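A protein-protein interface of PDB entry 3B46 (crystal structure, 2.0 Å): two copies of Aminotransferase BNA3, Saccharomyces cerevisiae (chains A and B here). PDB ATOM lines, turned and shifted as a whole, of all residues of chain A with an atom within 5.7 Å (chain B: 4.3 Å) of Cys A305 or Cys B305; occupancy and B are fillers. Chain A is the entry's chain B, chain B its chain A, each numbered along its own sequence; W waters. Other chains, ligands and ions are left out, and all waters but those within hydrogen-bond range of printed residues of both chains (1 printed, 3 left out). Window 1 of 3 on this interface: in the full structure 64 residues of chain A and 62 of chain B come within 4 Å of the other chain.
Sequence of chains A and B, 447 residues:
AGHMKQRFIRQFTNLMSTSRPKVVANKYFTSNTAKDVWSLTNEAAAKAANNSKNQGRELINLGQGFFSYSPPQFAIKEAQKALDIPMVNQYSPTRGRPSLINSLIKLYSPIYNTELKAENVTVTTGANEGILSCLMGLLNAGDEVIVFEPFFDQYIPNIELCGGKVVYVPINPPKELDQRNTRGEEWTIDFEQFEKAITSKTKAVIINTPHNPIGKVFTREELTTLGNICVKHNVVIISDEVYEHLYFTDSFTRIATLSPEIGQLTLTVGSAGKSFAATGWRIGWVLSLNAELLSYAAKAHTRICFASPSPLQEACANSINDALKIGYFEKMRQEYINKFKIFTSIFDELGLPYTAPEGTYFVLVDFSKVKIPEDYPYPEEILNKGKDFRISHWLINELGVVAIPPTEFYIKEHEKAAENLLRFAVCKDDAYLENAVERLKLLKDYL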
ATOM      1  N   THR A 125     -11.603 -20.384  21.555  1.00  0.00           N
ATOM      2  CA  THR A 125     -12.038 -21.343  20.554  1.00  0.00           C
ATOM      3  C   THR A 125     -12.252 -22.687  21.224  1.00  0.00           C
ATOM      4  O   THR A 125     -11.466 -23.642  21.076  1.00  0.00           O
ATOM      5  CB  THR A 125     -11.006 -21.363  19.410  1.00  0.00           C
ATOM      6  OG1 THR A 125     -10.962 -20.031  18.846  1.00  0.00           O
ATOM      7  CG2 THR A 125     -11.394 -22.378  18.292  1.00  0.00           C
ATOM      8  N   ASN A 128     -11.313 -26.212  25.591  1.00  0.00           N
ATOM      9  CA  ASN A 128      -9.959 -26.778  25.611  1.00  0.00           C
ATOM     10  C   ASN A 128      -8.881 -25.752  25.331  1.00  0.00           C
ATOM     11  O   ASN A 128      -7.907 -25.633  26.088  1.00  0.00           O
ATOM     12  CB  ASN A 128      -9.789 -27.965  24.635  1.00  0.00           C
ATOM     13  CG  ASN A 128     -10.530 -27.788  23.310  1.00  0.00           C
ATOM     14  OD1 ASN A 128     -10.606 -26.682  22.731  1.00  0.00           O
ATOM     15  ND2 ASN A 128     -11.080 -28.911  22.804  1.00  0.00           N
ATOM     16  N   GLU A 129      -9.046 -25.004  24.248  1.00  0.00           N
ATOM     17  CA  GLU A 129      -8.059 -23.993  23.910  1.00  0.00           C
ATOM     18  C   GLU A 129      -8.178 -22.779  24.883  1.00  0.00           C
ATOM     19  O   GLU A 129      -7.237 -22.007  25.027  1.00  0.00           O
ATOM     20  CB  GLU A 129      -8.207 -23.564  22.446  1.00  0.00           C
ATOM     21  CG  GLU A 129      -7.120 -22.577  22.000  1.00  0.00           C
ATOM     22  CD  GLU A 129      -7.594 -21.113  22.126  1.00  0.00           C
ATOM     23  OE1 GLU A 129      -6.782 -20.177  21.994  1.00  0.00           O
ATOM     24  OE2 GLU A 129      -8.804 -20.927  22.341  1.00  0.00           O
ATOM     25  N   LEU A 132      -6.056 -23.806  27.712  1.00  0.00           N
ATOM     26  CA  LEU A 132      -4.684 -23.694  27.226  1.00  0.00           C
ATOM     27  C   LEU A 132      -4.254 -22.221  27.312  1.00  0.00           C
ATOM     28  O   LEU A 132      -3.118 -21.900  27.659  1.00  0.00           O
ATOM     29  CB  LEU A 132      -4.605 -24.122  25.745  1.00  0.00           C
ATOM     30  CG  LEU A 132      -3.312 -24.732  25.154  1.00  0.00           C
ATOM     31  CD1 LEU A 132      -3.170 -24.440  23.636  1.00  0.00           C
ATOM     32  CD2 LEU A 132      -2.139 -24.219  25.882  1.00  0.00           C
ATOM     33  N   GLN A 154      -6.610 -33.652  27.876  1.00  0.00           N
ATOM     34  CA  GLN A 154      -5.958 -32.494  27.309  1.00  0.00           C
ATOM     35  C   GLN A 154      -5.199 -31.659  28.339  1.00  0.00           C
ATOM     36  O   GLN A 154      -4.280 -30.944  27.968  1.00  0.00           O
ATOM     37  CB  GLN A 154      -7.003 -31.613  26.585  1.00  0.00           C
ATOM     38  CG  GLN A 154      -6.413 -30.610  25.580  1.00  0.00           C
ATOM     39  CD  GLN A 154      -6.135 -31.234  24.207  1.00  0.00           C
ATOM     40  OE1 GLN A 154      -6.037 -30.530  23.203  1.00  0.00           O
ATOM     41  NE2 GLN A 154      -6.012 -32.547  24.168  1.00  0.00           N
ATOM     42  N   ARG A 282     -16.673 -25.146  18.500  1.00  0.00           N
ATOM     43  CA  ARG A 282     -15.403 -24.664  19.032  1.00  0.00           C
ATOM     44  C   ARG A 282     -15.498 -23.203  19.524  1.00  0.00           C
ATOM     45  O   ARG A 282     -14.761 -22.331  19.079  1.00  0.00           O
ATOM     46  CB  ARG A 282     -14.272 -24.815  17.992  1.00  0.00           C
ATOM     47  CG  ARG A 282     -14.368 -26.093  17.100  1.00  0.00           C
ATOM     48  CD  ARG A 282     -14.394 -27.394  17.888  1.00  0.00           C
ATOM     49  NE  ARG A 282     -13.325 -27.442  18.875  1.00  0.00           N
ATOM     50  CZ  ARG A 282     -13.523 -27.696  20.171  1.00  0.00           C
ATOM     51  NH1 ARG A 282     -14.748 -27.950  20.636  1.00  0.00           N
ATOM     52  NH2 ARG A 282     -12.511 -27.633  21.015  1.00  0.00           N
ATOM     53  N   ALA A 300      -2.907 -14.622  25.595  1.00  0.00           N
ATOM     54  CA  ALA A 300      -2.440 -15.898  25.104  1.00  0.00           C
ATOM     55  C   ALA A 300      -3.327 -16.333  23.940  1.00  0.00           C
ATOM     56  O   ALA A 300      -2.814 -16.742  22.890  1.00  0.00           O
ATOM     57  CB  ALA A 300      -2.483 -16.933  26.232  1.00  0.00           C
ATOM     58  N   HIS A 301      -4.650 -16.244  24.125  1.00  0.00           N
ATOM     59  CA  HIS A 301      -5.602 -16.618  23.087  1.00  0.00           C
ATOM     60  C   HIS A 301      -5.326 -15.849  21.797  1.00  0.00           C
ATOM     61  O   HIS A 301      -5.379 -16.415  20.702  1.00  0.00           O
ATOM     62  CB  HIS A 301      -7.042 -16.367  23.541  1.00  0.00           C
ATOM     63  CG  HIS A 301      -8.062 -16.641  22.481  1.00  0.00           C
ATOM     64  ND1 HIS A 301      -8.299 -17.907  21.987  1.00  0.00           N
ATOM     65  CD2 HIS A 301      -8.848 -15.803  21.760  1.00  0.00           C
ATOM     66  CE1 HIS A 301      -9.180 -17.835  21.007  1.00  0.00           C
ATOM     67  NE2 HIS A 301      -9.524 -16.570  20.845  1.00  0.00           N
ATOM     68  N   THR A 302      -5.055 -14.549  21.937  1.00  0.00           N
ATOM     69  CA  THR A 302      -4.730 -13.693  20.806  1.00  0.00           C
ATOM     70  C   THR A 302      -3.505 -14.248  20.045  1.00  0.00           C
ATOM     71  O   THR A 302      -3.459 -14.205  18.813  1.00  0.00           O
ATOM     72  CB  THR A 302      -4.342 -12.263  21.269  1.00  0.00           C
ATOM     73  OG1 THR A 302      -5.465 -11.629  21.888  1.00  0.00           O
ATOM     74  CG2 THR A 302      -3.900 -11.446  20.097  1.00  0.00           C
ATOM     75  N   ARG A 303      -2.518 -14.745  20.780  1.00  0.00           N
ATOM     76  CA  ARG A 303      -1.306 -15.276  20.156  1.00  0.00           C
ATOM     77  C   ARG A 303      -1.459 -16.719  19.683  1.00  0.00           C
ATOM     78  O   ARG A 303      -0.676 -17.181  18.850  1.00  0.00           O
ATOM     79  CB  ARG A 303      -0.113 -15.213  21.119  1.00  0.00           C
ATOM     80  CG  ARG A 303       0.131 -13.867  21.783  1.00  0.00           C
ATOM     81  CD  ARG A 303       0.284 -12.740  20.775  1.00  0.00           C
ATOM     82  NE  ARG A 303       0.751 -11.489  21.390  1.00  0.00           N
ATOM     83  CZ  ARG A 303       0.116 -10.820  22.360  1.00  0.00           C
ATOM     84  NH1 ARG A 303       0.638  -9.694  22.838  1.00  0.00           N
ATOM     85  NH2 ARG A 303      -1.037 -11.260  22.859  1.00  0.00           N
ATOM     86  N   ILE A 304      -2.443 -17.440  20.210  1.00  0.00           N
ATOM     87  CA  ILE A 304      -2.652 -18.832  19.786  1.00  0.00           C
ATOM     88  C   ILE A 304      -3.557 -18.948  18.550  1.00  0.00           C
ATOM     89  O   ILE A 304      -3.156 -19.530  17.530  1.00  0.00           O
ATOM     90  CB  ILE A 304      -3.256 -19.672  20.944  1.00  0.00           C
ATOM     91  CG1 ILE A 304      -2.236 -19.794  22.071  1.00  0.00           C
ATOM     92  CG2 ILE A 304      -3.657 -21.054  20.465  1.00  0.00           C
ATOM     93  CD1 ILE A 304      -2.847 -20.413  23.362  1.00  0.00           C
ATOM     94  N   CYS A 305      -4.772 -18.397  18.639  1.00  0.00           N
ATOM     95  CA  CYS A 305      -5.760 -18.460  17.549  1.00  0.00           C
ATOM     96  C   CYS A 305      -6.196 -17.111  16.973  1.00  0.00           C
ATOM     97  O   CYS A 305      -6.963 -17.078  16.017  1.00  0.00           O
ATOM     98  CB  CYS A 305      -7.052 -19.114  18.008  1.00  0.00           C
ATOM     99  SG  CYS A 305      -7.037 -20.809  18.504  1.00  0.00           S
ATOM    100  N   PHE A 306      -5.737 -16.026  17.586  1.00  0.00           N
ATOM    101  CA  PHE A 306      -6.087 -14.659  17.201  1.00  0.00           C
ATOM    102  C   PHE A 306      -7.558 -14.279  17.462  1.00  0.00           C
ATOM    103  O   PHE A 306      -7.841 -13.327  18.215  1.00  0.00           O
ATOM    104  CB  PHE A 306      -5.729 -14.396  15.742  1.00  0.00           C
ATOM    105  CG  PHE A 306      -5.956 -12.979  15.333  1.00  0.00           C
ATOM    106  CD1 PHE A 306      -5.511 -11.935  16.150  1.00  0.00           C
ATOM    107  CD2 PHE A 306      -6.608 -12.677  14.145  1.00  0.00           C
ATOM    108  CE1 PHE A 306      -5.712 -10.601  15.792  1.00  0.00           C
ATOM    109  CE2 PHE A 306      -6.819 -11.345  13.766  1.00  0.00           C
ATOM    110  CZ  PHE A 306      -6.367 -10.299  14.599  1.00  0.00           C
ATOM    111  N   ALA A 307      -8.493 -15.011  16.857  1.00  0.00           N
ATOM    112  CA  ALA A 307      -9.925 -14.753  17.043  1.00  0.00           C
ATOM    113  C   ALA A 307     -10.698 -16.036  16.830  1.00  0.00           C
ATOM    114  O   ALA A 307     -10.315 -16.870  16.008  1.00  0.00           O
ATOM    115  CB  ALA A 307     -10.431 -13.671  16.046  1.00  0.00           C
ATOM    116  N   SER A 308     -11.801 -16.180  17.558  1.00  0.00           N
ATOM    117  CA  SER A 308     -12.629 -17.367  17.464  1.00  0.00           C
ATOM    118  C   SER A 308     -13.669 -17.226  16.359  1.00  0.00           C
ATOM    119  O   SER A 308     -14.046 -16.109  16.003  1.00  0.00           O
ATOM    120  CB  SER A 308     -13.279 -17.633  18.812  1.00  0.00           C
ATOM    121  OG  SER A 308     -12.271 -17.826  19.788  1.00  0.00           O
ATOM    122  N   THR B 125      -7.121 -24.608  12.541  1.00  0.00           N
ATOM    123  CA  THR B 125      -8.083 -23.547  12.818  1.00  0.00           C
ATOM    124  C   THR B 125      -7.546 -22.222  12.337  1.00  0.00           C
ATOM    125  O   THR B 125      -7.168 -21.344  13.116  1.00  0.00           O
ATOM    126  CB  THR B 125      -8.426 -23.537  14.303  1.00  0.00           C
ATOM    127  OG1 THR B 125      -8.891 -24.855  14.651  1.00  0.00           O
ATOM    128  CG2 THR B 125      -9.575 -22.512  14.602  1.00  0.00           C
ATOM    129  N   ASN B 128      -3.017 -19.063  10.781  1.00  0.00           N
ATOM    130  CA  ASN B 128      -2.171 -18.665  11.892  1.00  0.00           C
ATOM    131  C   ASN B 128      -1.951 -19.769  12.896  1.00  0.00           C
ATOM    132  O   ASN B 128      -0.801 -20.025  13.308  1.00  0.00           O
ATOM    133  CB  ASN B 128      -2.669 -17.368  12.601  1.00  0.00           C
ATOM    134  CG  ASN B 128      -4.141 -17.409  13.029  1.00  0.00           C
ATOM    135  OD1 ASN B 128      -4.802 -18.475  13.111  1.00  0.00           O
ATOM    136  ND2 ASN B 128      -4.675 -16.210  13.318  1.00  0.00           N
ATOM    137  N   GLU B 129      -3.024 -20.443  13.310  1.00  0.00           N
ATOM    138  CA  GLU B 129      -2.815 -21.518  14.264  1.00  0.00           C
ATOM    139  C   GLU B 129      -2.202 -22.758  13.533  1.00  0.00           C
ATOM    140  O   GLU B 129      -1.637 -23.644  14.165  1.00  0.00           O
ATOM    141  CB  GLU B 129      -4.115 -21.873  14.969  1.00  0.00           C
ATOM    142  CG  GLU B 129      -3.915 -22.940  16.016  1.00  0.00           C
ATOM    143  CD  GLU B 129      -4.361 -24.292  15.525  1.00  0.00           C
ATOM    144  OE1 GLU B 129      -4.118 -25.281  16.240  1.00  0.00           O
ATOM    145  OE2 GLU B 129      -4.963 -24.355  14.431  1.00  0.00           O
ATOM    146  N   ARG B 282     -12.010 -19.226  10.352  1.00  0.00           N
ATOM    147  CA  ARG B 282     -10.948 -19.913  11.105  1.00  0.00           C
ATOM    148  C   ARG B 282     -10.763 -21.369  10.659  1.00  0.00           C
ATOM    149  O   ARG B 282     -10.854 -22.290  11.481  1.00  0.00           O
ATOM    150  CB  ARG B 282     -11.214 -19.904  12.625  1.00  0.00           C
ATOM    151  CG  ARG B 282     -11.754 -18.552  13.225  1.00  0.00           C
ATOM    152  CD  ARG B 282     -11.034 -17.354  12.661  1.00  0.00           C
ATOM    153  NE  ARG B 282      -9.607 -17.407  12.945  1.00  0.00           N
ATOM    154  CZ  ARG B 282      -8.655 -17.152  12.052  1.00  0.00           C
ATOM    155  NH1 ARG B 282      -8.968 -16.821  10.809  1.00  0.00           N
ATOM    156  NH2 ARG B 282      -7.387 -17.217  12.411  1.00  0.00           N
ATOM    157  N   HIS B 301      -1.407 -29.565  16.607  1.00  0.00           N
ATOM    158  CA  HIS B 301      -2.749 -29.028  16.420  1.00  0.00           C
ATOM    159  C   HIS B 301      -3.709 -29.737  17.356  1.00  0.00           C
ATOM    160  O   HIS B 301      -4.573 -29.097  17.947  1.00  0.00           O
ATOM    161  CB  HIS B 301      -3.239 -29.203  14.979  1.00  0.00           C
ATOM    162  CG  HIS B 301      -4.632 -28.703  14.759  1.00  0.00           C
ATOM    163  ND1 HIS B 301      -4.985 -27.380  14.941  1.00  0.00           N
ATOM    164  CD2 HIS B 301      -5.764 -29.346  14.392  1.00  0.00           C
ATOM    165  CE1 HIS B 301      -6.272 -27.235  14.692  1.00  0.00           C
ATOM    166  NE2 HIS B 301      -6.769 -28.411  14.357  1.00  0.00           N
ATOM    167  N   ARG B 303      -3.116 -30.984  20.235  1.00  0.00           N
ATOM    168  CA  ARG B 303      -2.875 -30.538  21.596  1.00  0.00           C
ATOM    169  C   ARG B 303      -3.200 -29.063  21.797  1.00  0.00           C
ATOM    170  O   ARG B 303      -3.331 -28.614  22.929  1.00  0.00           O
ATOM    171  CB  ARG B 303      -1.411 -30.802  22.000  1.00  0.00           C
ATOM    172  CG  ARG B 303      -0.973 -32.281  21.867  1.00  0.00           C
ATOM    173  CD  ARG B 303      -1.804 -33.166  22.785  1.00  0.00           C
ATOM    174  NE  ARG B 303      -1.984 -34.516  22.263  1.00  0.00           N
ATOM    175  CZ  ARG B 303      -3.058 -35.278  22.500  1.00  0.00           C
ATOM    176  NH1 ARG B 303      -3.137 -36.494  21.973  1.00  0.00           N
ATOM    177  NH2 ARG B 303      -4.067 -34.827  23.250  1.00  0.00           N
ATOM    178  N   ILE B 304      -3.305 -28.307  20.718  1.00  0.00           N
ATOM    179  CA  ILE B 304      -3.610 -26.886  20.853  1.00  0.00           C
ATOM    180  C   ILE B 304      -5.114 -26.654  20.780  1.00  0.00           C
ATOM    181  O   ILE B 304      -5.721 -26.136  21.720  1.00  0.00           O
ATOM    182  CB  ILE B 304      -2.928 -26.061  19.752  1.00  0.00           C
ATOM    183  CG1 ILE B 304      -1.402 -26.200  19.860  1.00  0.00           C
ATOM    184  CG2 ILE B 304      -3.316 -24.590  19.885  1.00  0.00           C
ATOM    185  CD1 ILE B 304      -0.623 -25.385  18.800  1.00  0.00           C
ATOM    186  N   CYS B 305      -5.719 -27.083  19.674  1.00  0.00           N
ATOM    187  CA  CYS B 305      -7.147 -26.883  19.437  1.00  0.00           C
ATOM    188  C   CYS B 305      -8.013 -28.132  19.460  1.00  0.00           C
ATOM    189  O   CYS B 305      -9.228 -28.050  19.625  1.00  0.00           O
ATOM    190  CB  CYS B 305      -7.351 -26.194  18.084  1.00  0.00           C
ATOM    191  SG  CYS B 305      -6.970 -24.433  18.049  1.00  0.00           S
ATOM    192  N   PHE B 306      -7.363 -29.273  19.258  1.00  0.00           N
ATOM    193  CA  PHE B 306      -7.978 -30.598  19.189  1.00  0.00           C
ATOM    194  C   PHE B 306      -8.607 -30.866  17.834  1.00  0.00           C
ATOM    195  O   PHE B 306      -8.149 -31.747  17.092  1.00  0.00           O
ATOM    196  CB  PHE B 306      -9.023 -30.825  20.270  1.00  0.00           C
ATOM    197  CG  PHE B 306      -9.571 -32.210  20.249  1.00  0.00           C
ATOM    198  CD1 PHE B 306      -8.733 -33.295  20.502  1.00  0.00           C
ATOM    199  CD2 PHE B 306     -10.891 -32.450  19.882  1.00  0.00           C
ATOM    200  CE1 PHE B 306      -9.197 -34.598  20.383  1.00  0.00           C
ATOM    201  CE2 PHE B 306     -11.367 -33.747  19.758  1.00  0.00           C
ATOM    202  CZ  PHE B 306     -10.515 -34.828  20.009  1.00  0.00           C
ATOM    203  N   ALA B 307      -9.663 -30.123  17.514  1.00  0.00           N
ATOM    204  CA  ALA B 307     -10.348 -30.251  16.224  1.00  0.00           C
ATOM    205  C   ALA B 307     -10.799 -28.853  15.758  1.00  0.00           C
ATOM    206  O   ALA B 307     -11.048 -27.961  16.580  1.00  0.00           O
ATOM    207  CB  ALA B 307     -11.554 -31.196  16.349  1.00  0.00           C
HETATM  208  O   HOH W   1      -7.840 -19.464  14.718  1.00  0.00           O
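The backbone NH (N) of Thr B125 is in hydrogen-bond range of the side-chain carboxylate (OE2) of Glu B129 (2.9 Å).
OD1 of Asn B128 sits at hydrogen-bond distance from NH2 of Arg B282.
N of Phe B306 is in hydrogen-bond range of O of His B301 (3.1 Å).
The backbone NH of Thr A125 sits at hydrogen-bond distance from the side-chain carboxylate of Glu A129 (3.0 Å).
The side-chain hydroxyl (OG1) of Thr A125 lies within hydrogen-bond range of the side-chain hydroxyl (OG) of Ser A308.
OG of Ser A308 sits at hydrogen-bond distance from NE2 of His A301, 3.2 Å away.
Among the printed residues, pairs that only touch across the chains: Phe A306 with Asn B128 (3.2 Å), Arg A282 with Cys B305 (3.6 Å), Ile A304 with Ile B304 (3.6 Å), Ile A304 with Glu B129 (3.6 Å), Leu A132 with Ile B304 (3.6 Å), Cys A305 with Arg B282 (3.6 Å), Cys A305 with Asn B128 (3.6 Å), Glu A129 with Ile B304 (3.6 Å), Asn A128 with Cys B305 (3.7 Å), Asn A128 with Phe B306 (3.8 Å) and Ser A308 with Arg B282 (3.9 Å).
Water W1 lies within hydrogen-bond range of O of Thr B125 (2.6 Å), O of Cys A305 (2.9 Å) and NE of Arg B282 (3.2 Å).
Asn A128 touches Phe B306, and with the chains exchanged Phe A306 touches Asn B128.
Glu A129 touches Ile B304, and with the chains exchanged Ile A304 touches Glu B129.
Arg A282 touches Ala B307, and with the chains exchanged Ala A307 touches Arg B282.
Ile B304 touches its own counterpart, Ile A304.
Hydrophobic or aromatic side chains of chain A that line the printed part of chain B: Leu A132, Ile A304 and Phe A306.
Of the 10 printed residues of chain B, 8 touch a printed residue of chain A.
Printed residues of chain B that touch a printed residue of chain A: Asn B128, Glu B129, Arg B282, Arg B303, Ile B304, Cys B305, Phe B306 and Ala B307.
Hydrophobic or aromatic side chains of chain B that line the printed part of chain A: Ile B304 and Phe B306.
Among the printed residues, no Asp or Glu carboxylate lies within 4 Å of a Lys or Arg side-chain nitrogen of the other chain.
Of the printed residues of chain B, Asn A128 touches Cys B305 (3.7 Å) and Phe B306 (3.8 Å).
Printed residues of chain B within 4 Å of Arg A282: Cys B305 (3.6 Å) and Ala B307 (3.3 Å).
Arg A303 touches none of the printed residues of chain B.
His B301 touches none of the printed residues of chain A.
The nearest printed residue of chain B that does not touch Cys A305 is Glu B129 (4.5 Å).
The guanidinium group (NE) of Arg B282 is in hydrogen-bond range of the backbone carbonyl oxygen (O) of Ala A307, 3.2 Å away.
NE2 of Gln A154 lies close to NH2 of Arg B303, 3.1 Å away.
The side-chain sulfur (SG) of Cys B305 is in hydrogen-bond range of the side-chain sulfur (SG) of Cys A305, 3.7 Å away.
The guanidinium group (NE) of Arg A282 sits at hydrogen-bond distance from the backbone carbonyl oxygen (O) of Ala B307.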
